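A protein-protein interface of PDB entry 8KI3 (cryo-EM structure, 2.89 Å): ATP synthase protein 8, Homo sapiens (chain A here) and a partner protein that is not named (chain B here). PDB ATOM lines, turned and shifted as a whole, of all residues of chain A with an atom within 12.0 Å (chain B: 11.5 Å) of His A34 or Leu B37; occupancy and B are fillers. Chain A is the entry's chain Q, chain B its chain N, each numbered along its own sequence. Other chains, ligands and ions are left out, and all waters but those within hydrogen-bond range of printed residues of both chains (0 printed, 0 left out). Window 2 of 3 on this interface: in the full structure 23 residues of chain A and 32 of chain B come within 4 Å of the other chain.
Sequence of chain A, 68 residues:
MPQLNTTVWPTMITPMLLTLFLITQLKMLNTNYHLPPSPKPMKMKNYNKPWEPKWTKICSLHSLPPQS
Hydrophobic or aromatic side chains of chain A that line the printed part of chain B: Tyr A33 and His A34. Of the 17 printed residues of chain B, 5 touch a printed residue of chain A. Printed residues of chain B that touch a printed residue of chain A: Thr B33, Lys B35, Leu B37, Gln B47 and Lys B51. Hydrophobic or aromatic side chains of chain B that line the printed part of chain A: Leu B37. Among the printed residues, no Asp or Glu carboxylate lies within 4 Å of a Lys or Arg side-chain nitrogen of the other chain.
Of the printed residues of chain B, Asn A30 touches Thr B33 (3.4 Å) and Lys B35 (3.3 Å). Printed residues of chain B within 4 Å of Thr A31: Gln B47 (3.7 Å). Of the printed residues of chain B, Tyr A33 touches Gln B47 and Lys B51. Of the printed residues of chain B, His A34 touches Leu B37 (3.6 Å). Leu A35 touches none of the printed residues of chain B. No residue of chain B comes within 4 Å of Pro A36. Of the printed residues of chain A, Thr B33 touches Asn A30. Of the printed residues of chain A, Lys B35 touches Asn A30. Leu B37 touches one residue of chain A. Ile B38 touches none of the printed residues of chain A. The nearest residue of chain B that does not touch His A34 is Tyr B36 (7.0 Å).
Among the printed residues, pairs that only touch across the chains: Asn A30 with Lys B35 (3.3 Å), His A34 with Leu B37 (3.6 Å) and Thr A31 with Gln B47 (3.7 Å).
The side-chain amide nitrogen (ND2) of Asn A30 is in hydrogen-bond range of the side-chain hydroxyl (OG1) of Thr B33, at 3.4 Å. O of Gln B47 is in hydrogen-bond range of OH of Tyr A33 (2.7 Å). The backbone NH (N) of Lys B51 sits at hydrogen-bond distance from the side-chain hydroxyl (OH) of Tyr A33 (3.2 Å).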
ATOM      1  N   MET A  28     -28.106 -21.951  10.702  1.00  0.00           N
ATOM      2  CA  MET A  28     -28.484 -22.353   9.354  1.00  0.00           C
ATOM      3  C   MET A  28     -29.547 -21.428   8.785  1.00  0.00           C
ATOM      4  O   MET A  28     -29.505 -21.088   7.598  1.00  0.00           O
ATOM      5  CB  MET A  28     -28.981 -23.794   9.345  1.00  0.00           C
ATOM      6  CG  MET A  28     -27.883 -24.820   9.333  1.00  0.00           C
ATOM      7  SD  MET A  28     -26.553 -24.368   8.224  1.00  0.00           S
ATOM      8  CE  MET A  28     -25.250 -25.408   8.854  1.00  0.00           C
ATOM      9  N   LEU A  29     -30.503 -21.006   9.611  1.00  0.00           N
ATOM     10  CA  LEU A  29     -31.508 -20.051   9.168  1.00  0.00           C
ATOM     11  C   LEU A  29     -30.904 -18.735   8.711  1.00  0.00           C
ATOM     12  O   LEU A  29     -31.601 -17.941   8.075  1.00  0.00           O
ATOM     13  CB  LEU A  29     -32.512 -19.789  10.286  1.00  0.00           C
ATOM     14  CG  LEU A  29     -33.525 -20.903  10.511  1.00  0.00           C
ATOM     15  CD1 LEU A  29     -34.443 -20.547  11.654  1.00  0.00           C
ATOM     16  CD2 LEU A  29     -34.315 -21.133   9.247  1.00  0.00           C
ATOM     17  N   ASN A  30     -29.636 -18.485   9.019  1.00  0.00           N
ATOM     18  CA  ASN A  30     -28.939 -17.297   8.562  1.00  0.00           C
ATOM     19  C   ASN A  30     -28.213 -17.520   7.247  1.00  0.00           C
ATOM     20  O   ASN A  30     -27.674 -16.566   6.683  1.00  0.00           O
ATOM     21  CB  ASN A  30     -27.949 -16.831   9.626  1.00  0.00           C
ATOM     22  CG  ASN A  30     -27.913 -15.334   9.760  1.00  0.00           C
ATOM     23  OD1 ASN A  30     -28.148 -14.611   8.797  1.00  0.00           O
ATOM     24  ND2 ASN A  30     -27.620 -14.855  10.960  1.00  0.00           N
ATOM     25  N   THR A  31     -28.191 -18.750   6.748  1.00  0.00           N
ATOM     26  CA  THR A  31     -27.582 -19.082   5.463  1.00  0.00           C
ATOM     27  C   THR A  31     -28.707 -19.187   4.441  1.00  0.00           C
ATOM     28  O   THR A  31     -29.408 -20.200   4.378  1.00  0.00           O
ATOM     29  CB  THR A  31     -26.787 -20.379   5.561  1.00  0.00           C
ATOM     30  OG1 THR A  31     -25.582 -20.146   6.295  1.00  0.00           O
ATOM     31  CG2 THR A  31     -26.429 -20.889   4.186  1.00  0.00           C
ATOM     32  N   ASN A  32     -28.893 -18.135   3.649  1.00  0.00           N
ATOM     33  CA  ASN A  32     -29.973 -18.074   2.676  1.00  0.00           C
ATOM     34  C   ASN A  32     -29.415 -17.965   1.266  1.00  0.00           C
ATOM     35  O   ASN A  32     -28.402 -17.300   1.035  1.00  0.00           O
ATOM     36  CB  ASN A  32     -30.907 -16.898   2.947  1.00  0.00           C
ATOM     37  CG  ASN A  32     -31.693 -17.063   4.224  1.00  0.00           C
ATOM     38  OD1 ASN A  32     -31.549 -16.280   5.158  1.00  0.00           O
ATOM     39  ND2 ASN A  32     -32.527 -18.092   4.273  1.00  0.00           N
ATOM     40  N   TYR A  33     -30.092 -18.619   0.332  1.00  0.00           N
ATOM     41  CA  TYR A  33     -29.706 -18.650  -1.074  1.00  0.00           C
ATOM     42  C   TYR A  33     -30.775 -17.915  -1.871  1.00  0.00           C
ATOM     43  O   TYR A  33     -31.858 -18.452  -2.114  1.00  0.00           O
ATOM     44  CB  TYR A  33     -29.548 -20.085  -1.558  1.00  0.00           C
ATOM     45  CG  TYR A  33     -28.612 -20.909  -0.716  1.00  0.00           C
ATOM     46  CD1 TYR A  33     -27.264 -20.972  -1.013  1.00  0.00           C
ATOM     47  CD2 TYR A  33     -29.075 -21.620   0.375  1.00  0.00           C
ATOM     48  CE1 TYR A  33     -26.409 -21.718  -0.252  1.00  0.00           C
ATOM     49  CE2 TYR A  33     -28.223 -22.368   1.143  1.00  0.00           C
ATOM     50  CZ  TYR A  33     -26.892 -22.413   0.824  1.00  0.00           C
ATOM     51  OH  TYR A  33     -26.031 -23.158   1.584  1.00  0.00           O
ATOM     52  N   HIS A  34     -30.466 -16.691  -2.277  1.00  0.00           N
ATOM     53  CA  HIS A  34     -31.411 -15.895  -3.040  1.00  0.00           C
ATOM     54  C   HIS A  34     -31.559 -16.443  -4.452  1.00  0.00           C
ATOM     55  O   HIS A  34     -30.614 -16.973  -5.039  1.00  0.00           O
ATOM     56  CB  HIS A  34     -30.951 -14.446  -3.099  1.00  0.00           C
ATOM     57  CG  HIS A  34     -29.681 -14.259  -3.863  1.00  0.00           C
ATOM     58  ND1 HIS A  34     -29.629 -14.296  -5.238  1.00  0.00           N
ATOM     59  CD2 HIS A  34     -28.414 -14.049  -3.443  1.00  0.00           C
ATOM     60  CE1 HIS A  34     -28.384 -14.109  -5.633  1.00  0.00           C
ATOM     61  NE2 HIS A  34     -27.626 -13.956  -4.563  1.00  0.00           N
ATOM     62  N   LEU A  35     -32.761 -16.301  -5.001  1.00  0.00           N
ATOM     63  CA  LEU A  35     -33.014 -16.745  -6.359  1.00  0.00           C
ATOM     64  C   LEU A  35     -32.253 -15.861  -7.344  1.00  0.00           C
ATOM     65  O   LEU A  35     -32.066 -14.668  -7.099  1.00  0.00           O
ATOM     66  CB  LEU A  35     -34.505 -16.697  -6.672  1.00  0.00           C
ATOM     67  CG  LEU A  35     -35.412 -17.756  -6.047  1.00  0.00           C
ATOM     68  CD1 LEU A  35     -35.678 -17.452  -4.586  1.00  0.00           C
ATOM     69  CD2 LEU A  35     -36.713 -17.864  -6.812  1.00  0.00           C
ATOM     70  N   PRO A  36     -31.797 -16.417  -8.461  1.00  0.00           N
ATOM     71  CA  PRO A  36     -31.026 -15.624  -9.421  1.00  0.00           C
ATOM     72  C   PRO A  36     -31.915 -14.623 -10.135  1.00  0.00           C
ATOM     73  O   PRO A  36     -33.125 -14.847 -10.278  1.00  0.00           O
ATOM     74  CB  PRO A  36     -30.477 -16.678 -10.395  1.00  0.00           C
ATOM     75  CG  PRO A  36     -30.662 -17.990  -9.704  1.00  0.00           C
ATOM     76  CD  PRO A  36     -31.877 -17.829  -8.860  1.00  0.00           C
ATOM     77  N   PRO A  37     -31.357 -13.510 -10.594  1.00  0.00           N
ATOM     78  CA  PRO A  37     -32.148 -12.502 -11.301  1.00  0.00           C
ATOM     79  C   PRO A  37     -32.317 -12.884 -12.768  1.00  0.00           C
ATOM     80  O   PRO A  37     -31.880 -13.941 -13.215  1.00  0.00           O
ATOM     81  CB  PRO A  37     -31.314 -11.225 -11.146  1.00  0.00           C
ATOM     82  CG  PRO A  37     -30.166 -11.587 -10.235  1.00  0.00           C
ATOM     83  CD  PRO A  37     -29.981 -13.051 -10.377  1.00  0.00           C
ATOM     84  N   SER A  38     -32.967 -11.996 -13.515  1.00  0.00           N
ATOM     85  CA  SER A  38     -33.177 -12.202 -14.946  1.00  0.00           C
ATOM     86  C   SER A  38     -31.854 -12.249 -15.698  1.00  0.00           C
ATOM     87  O   SER A  38     -31.603 -13.171 -16.473  1.00  0.00           O
ATOM     88  CB  SER A  38     -34.065 -11.099 -15.522  1.00  0.00           C
ATOM     89  OG  SER A  38     -33.508  -9.821 -15.273  1.00  0.00           O
ATOM     90  N   THR B  33     -21.780 -16.694  10.133  1.00  0.00           N
ATOM     91  CA  THR B  33     -22.797 -16.333   9.162  1.00  0.00           C
ATOM     92  C   THR B  33     -22.741 -14.838   8.900  1.00  0.00           C
ATOM     93  O   THR B  33     -22.213 -14.065   9.702  1.00  0.00           O
ATOM     94  CB  THR B  33     -24.193 -16.719   9.643  1.00  0.00           C
ATOM     95  OG1 THR B  33     -24.425 -16.145  10.934  1.00  0.00           O
ATOM     96  CG2 THR B  33     -24.314 -18.221   9.743  1.00  0.00           C
ATOM     97  N   SER B  34     -23.299 -14.432   7.764  1.00  0.00           N
ATOM     98  CA  SER B  34     -23.323 -13.024   7.407  1.00  0.00           C
ATOM     99  C   SER B  34     -24.505 -12.756   6.493  1.00  0.00           C
ATOM    100  O   SER B  34     -24.866 -13.588   5.658  1.00  0.00           O
ATOM    101  CB  SER B  34     -22.028 -12.592   6.719  1.00  0.00           C
ATOM    102  OG  SER B  34     -22.052 -12.930   5.345  1.00  0.00           O
ATOM    103  N   LYS B  35     -25.099 -11.577   6.660  1.00  0.00           N
ATOM    104  CA  LYS B  35     -26.192 -11.137   5.808  1.00  0.00           C
ATOM    105  C   LYS B  35     -25.713 -10.599   4.469  1.00  0.00           C
ATOM    106  O   LYS B  35     -26.542 -10.366   3.585  1.00  0.00           O
ATOM    107  CB  LYS B  35     -27.013 -10.061   6.519  1.00  0.00           C
ATOM    108  CG  LYS B  35     -27.594 -10.494   7.850  1.00  0.00           C
ATOM    109  CD  LYS B  35     -28.860 -11.309   7.655  1.00  0.00           C
ATOM    110  CE  LYS B  35     -29.507 -11.655   8.986  1.00  0.00           C
ATOM    111  NZ  LYS B  35     -29.883 -10.444   9.763  1.00  0.00           N
ATOM    112  N   TYR B  36     -24.411 -10.394   4.301  1.00  0.00           N
ATOM    113  CA  TYR B  36     -23.904  -9.755   3.100  1.00  0.00           C
ATOM    114  C   TYR B  36     -24.103 -10.648   1.881  1.00  0.00           C
ATOM    115  O   TYR B  36     -24.556 -11.789   1.969  1.00  0.00           O
ATOM    116  CB  TYR B  36     -22.428  -9.409   3.264  1.00  0.00           C
ATOM    117  CG  TYR B  36     -22.207  -8.226   4.159  1.00  0.00           C
ATOM    118  CD1 TYR B  36     -21.008  -8.050   4.826  1.00  0.00           C
ATOM    119  CD2 TYR B  36     -23.206  -7.286   4.347  1.00  0.00           C
ATOM    120  CE1 TYR B  36     -20.809  -6.964   5.651  1.00  0.00           C
ATOM    121  CE2 TYR B  36     -23.018  -6.199   5.167  1.00  0.00           C
ATOM    122  CZ  TYR B  36     -21.819  -6.042   5.817  1.00  0.00           C
ATOM    123  OH  TYR B  36     -21.634  -4.955   6.637  1.00  0.00           O
ATOM    124  N   LEU B  37     -23.754 -10.100   0.724  1.00  0.00           N
ATOM    125  CA  LEU B  37     -23.916 -10.795  -0.542  1.00  0.00           C
ATOM    126  C   LEU B  37     -22.624 -11.403  -1.051  1.00  0.00           C
ATOM    127  O   LEU B  37     -22.663 -12.435  -1.726  1.00  0.00           O
ATOM    128  CB  LEU B  37     -24.463  -9.834  -1.599  1.00  0.00           C
ATOM    129  CG  LEU B  37     -25.178 -10.463  -2.785  1.00  0.00           C
ATOM    130  CD1 LEU B  37     -26.141 -11.504  -2.286  1.00  0.00           C
ATOM    131  CD2 LEU B  37     -25.908  -9.397  -3.559  1.00  0.00           C
ATOM    132  N   ILE B  38     -21.488 -10.786  -0.746  1.00  0.00           N
ATOM    133  CA  ILE B  38     -20.187 -11.299  -1.153  1.00  0.00           C
ATOM    134  C   ILE B  38     -19.259 -11.260   0.051  1.00  0.00           C
ATOM    135  O   ILE B  38     -18.725 -10.204   0.403  1.00  0.00           O
ATOM    136  CB  ILE B  38     -19.611 -10.490  -2.326  1.00  0.00           C
ATOM    137  CG1 ILE B  38     -20.526 -10.611  -3.540  1.00  0.00           C
ATOM    138  CG2 ILE B  38     -18.215 -10.969  -2.662  1.00  0.00           C
ATOM    139  CD1 ILE B  38     -20.044  -9.845  -4.729  1.00  0.00           C
ATOM    140  N   ASN B  39     -19.118 -12.400   0.734  1.00  0.00           N
ATOM    141  CA  ASN B  39     -18.352 -12.392   2.010  1.00  0.00           C
ATOM    142  C   ASN B  39     -16.942 -12.960   1.840  1.00  0.00           C
ATOM    143  O   ASN B  39     -16.384 -12.842   0.731  1.00  0.00           O
ATOM    144  CB  ASN B  39     -19.098 -13.146   3.114  1.00  0.00           C
ATOM    145  CG  ASN B  39     -20.544 -13.429   2.767  1.00  0.00           C
ATOM    146  OD1 ASN B  39     -21.288 -12.523   2.395  1.00  0.00           O
ATOM    147  ND2 ASN B  39     -20.952 -14.681   2.889  1.00  0.00           N
ATOM    148  N   ASN B  40     -16.399 -13.555   2.906  1.00  0.00           N
ATOM    149  CA  ASN B  40     -15.036 -14.058   2.886  1.00  0.00           C
ATOM    150  C   ASN B  40     -14.988 -15.498   2.391  1.00  0.00           C
ATOM    151  O   ASN B  40     -16.005 -16.115   2.069  1.00  0.00           O
ATOM    152  CB  ASN B  40     -14.419 -13.958   4.273  1.00  0.00           C
ATOM    153  CG  ASN B  40     -15.353 -14.438   5.340  1.00  0.00           C
ATOM    154  OD1 ASN B  40     -16.506 -14.744   5.067  1.00  0.00           O
ATOM    155  ND2 ASN B  40     -14.865 -14.520   6.563  1.00  0.00           N
ATOM    156  N   ARG B  41     -13.771 -16.038   2.334  1.00  0.00           N
ATOM    157  CA  ARG B  41     -13.575 -17.369   1.779  1.00  0.00           C
ATOM    158  C   ARG B  41     -14.213 -18.440   2.645  1.00  0.00           C
ATOM    159  O   ARG B  41     -14.704 -19.443   2.120  1.00  0.00           O
ATOM    160  CB  ARG B  41     -12.087 -17.650   1.614  1.00  0.00           C
ATOM    161  CG  ARG B  41     -11.463 -16.995   0.408  1.00  0.00           C
ATOM    162  CD  ARG B  41      -9.965 -16.906   0.582  1.00  0.00           C
ATOM    163  NE  ARG B  41      -9.260 -16.915  -0.691  1.00  0.00           N
ATOM    164  CZ  ARG B  41      -7.946 -16.776  -0.811  1.00  0.00           C
ATOM    165  NH1 ARG B  41      -7.195 -16.616   0.268  1.00  0.00           N
ATOM    166  NH2 ARG B  41      -7.383 -16.796  -2.007  1.00  0.00           N
ATOM    167  N   LEU B  42     -14.210 -18.254   3.963  1.00  0.00           N
ATOM    168  CA  LEU B  42     -14.795 -19.251   4.850  1.00  0.00           C
ATOM    169  C   LEU B  42     -16.281 -19.420   4.572  1.00  0.00           C
ATOM    170  O   LEU B  42     -16.737 -20.500   4.186  1.00  0.00           O
ATOM    171  CB  LEU B  42     -14.558 -18.865   6.306  1.00  0.00           C
ATOM    172  CG  LEU B  42     -14.943 -19.949   7.305  1.00  0.00           C
ATOM    173  CD1 LEU B  42     -14.130 -21.190   7.045  1.00  0.00           C
ATOM    174  CD2 LEU B  42     -14.737 -19.468   8.719  1.00  0.00           C
ATOM    175  N   ILE B  43     -17.056 -18.348   4.746  1.00  0.00           N
ATOM    176  CA  ILE B  43     -18.491 -18.447   4.540  1.00  0.00           C
ATOM    177  C   ILE B  43     -18.840 -18.690   3.081  1.00  0.00           C
ATOM    178  O   ILE B  43     -19.948 -19.140   2.785  1.00  0.00           O
ATOM    179  CB  ILE B  43     -19.191 -17.187   5.065  1.00  0.00           C
ATOM    180  CG1 ILE B  43     -18.577 -16.763   6.387  1.00  0.00           C
ATOM    181  CG2 ILE B  43     -20.659 -17.447   5.268  1.00  0.00           C
ATOM    182  CD1 ILE B  43     -19.239 -15.568   6.988  1.00  0.00           C
ATOM    183  N   THR B  44     -17.928 -18.415   2.150  1.00  0.00           N
ATOM    184  CA  THR B  44     -18.207 -18.747   0.758  1.00  0.00           C
ATOM    185  C   THR B  44     -18.068 -20.239   0.518  1.00  0.00           C
ATOM    186  O   THR B  44     -18.832 -20.825  -0.256  1.00  0.00           O
ATOM    187  CB  THR B  44     -17.279 -17.977  -0.172  1.00  0.00           C
ATOM    188  OG1 THR B  44     -17.374 -16.577   0.108  1.00  0.00           O
ATOM    189  CG2 THR B  44     -17.666 -18.224  -1.613  1.00  0.00           C
ATOM    190  N   THR B  45     -17.093 -20.872   1.169  1.00  0.00           N
ATOM    191  CA  THR B  45     -16.937 -22.315   1.039  1.00  0.00           C
ATOM    192  C   THR B  45     -17.981 -23.054   1.859  1.00  0.00           C
ATOM    193  O   THR B  45     -18.485 -24.098   1.435  1.00  0.00           O
ATOM    194  CB  THR B  45     -15.536 -22.734   1.466  1.00  0.00           C
ATOM    195  OG1 THR B  45     -14.574 -21.875   0.848  1.00  0.00           O
ATOM    196  CG2 THR B  45     -15.267 -24.158   1.045  1.00  0.00           C
ATOM    197  N   GLN B  47     -21.125 -21.929   2.860  1.00  0.00           N
ATOM    198  CA  GLN B  47     -22.426 -21.801   2.220  1.00  0.00           C
ATOM    199  C   GLN B  47     -22.508 -22.593   0.930  1.00  0.00           C
ATOM    200  O   GLN B  47     -23.611 -22.842   0.440  1.00  0.00           O
ATOM    201  CB  GLN B  47     -22.747 -20.336   1.944  1.00  0.00           C
ATOM    202  CG  GLN B  47     -23.077 -19.540   3.183  1.00  0.00           C
ATOM    203  CD  GLN B  47     -23.613 -18.171   2.858  1.00  0.00           C
ATOM    204  OE1 GLN B  47     -23.944 -17.394   3.751  1.00  0.00           O
ATOM    205  NE2 GLN B  47     -23.705 -17.863   1.574  1.00  0.00           N
ATOM    206  N   TRP B  48     -21.371 -22.998   0.370  1.00  0.00           N
ATOM    207  CA  TRP B  48     -21.393 -23.881  -0.788  1.00  0.00           C
ATOM    208  C   TRP B  48     -21.573 -25.331  -0.364  1.00  0.00           C
ATOM    209  O   TRP B  48     -22.347 -26.072  -0.978  1.00  0.00           O
ATOM    210  CB  TRP B  48     -20.111 -23.717  -1.598  1.00  0.00           C
ATOM    211  CG  TRP B  48     -20.045 -24.618  -2.776  1.00  0.00           C
ATOM    212  CD1 TRP B  48     -20.704 -24.467  -3.955  1.00  0.00           C
ATOM    213  CD2 TRP B  48     -19.277 -25.815  -2.897  1.00  0.00           C
ATOM    214  NE1 TRP B  48     -20.394 -25.495  -4.805  1.00  0.00           N
ATOM    215  CE2 TRP B  48     -19.518 -26.338  -4.177  1.00  0.00           C
ATOM    216  CE3 TRP B  48     -18.407 -26.497  -2.046  1.00  0.00           C
ATOM    217  CZ2 TRP B  48     -18.924 -27.509  -4.627  1.00  0.00           C
ATOM    218  CZ3 TRP B  48     -17.818 -27.658  -2.493  1.00  0.00           C
ATOM    219  CH2 TRP B  48     -18.079 -28.153  -3.770  1.00  0.00           C
ATOM    220  N   LYS B  51     -24.971 -25.953   0.537  1.00  0.00           N
ATOM    221  CA  LYS B  51     -25.786 -26.043  -0.667  1.00  0.00           C
ATOM    222  C   LYS B  51     -25.648 -27.412  -1.312  1.00  0.00           C
ATOM    223  O   LYS B  51     -26.645 -28.033  -1.694  1.00  0.00           O
ATOM    224  CB  LYS B  51     -25.396 -24.944  -1.651  1.00  0.00           C
ATOM    225  CG  LYS B  51     -26.188 -24.968  -2.934  1.00  0.00           C
ATOM    226  CD  LYS B  51     -26.173 -23.617  -3.611  1.00  0.00           C
ATOM    227  CE  LYS B  51     -24.826 -23.335  -4.230  1.00  0.00           C
ATOM    228  NZ  LYS B  51     -24.486 -24.358  -5.249  1.00  0.00           N
ATOM    229  N   LYS B  55     -28.744 -30.308  -1.141  1.00  0.00           N
ATOM    230  CA  LYS B  55     -29.229 -30.841  -2.407  1.00  0.00           C
ATOM    231  C   LYS B  55     -29.059 -32.348  -2.501  1.00  0.00           C
ATOM    232  O   LYS B  55     -29.615 -32.963  -3.414  1.00  0.00           O
ATOM    233  CB  LYS B  55     -28.508 -30.177  -3.576  1.00  0.00           C
ATOM    234  CG  LYS B  55     -29.003 -28.789  -3.902  1.00  0.00           C
ATOM    235  CD  LYS B  55     -28.138 -28.143  -4.958  1.00  0.00           C
ATOM    236  CE  LYS B  55     -27.970 -29.061  -6.147  1.00  0.00           C
ATOM    237  NZ  LYS B  55     -29.287 -29.439  -6.723  1.00  0.00           N
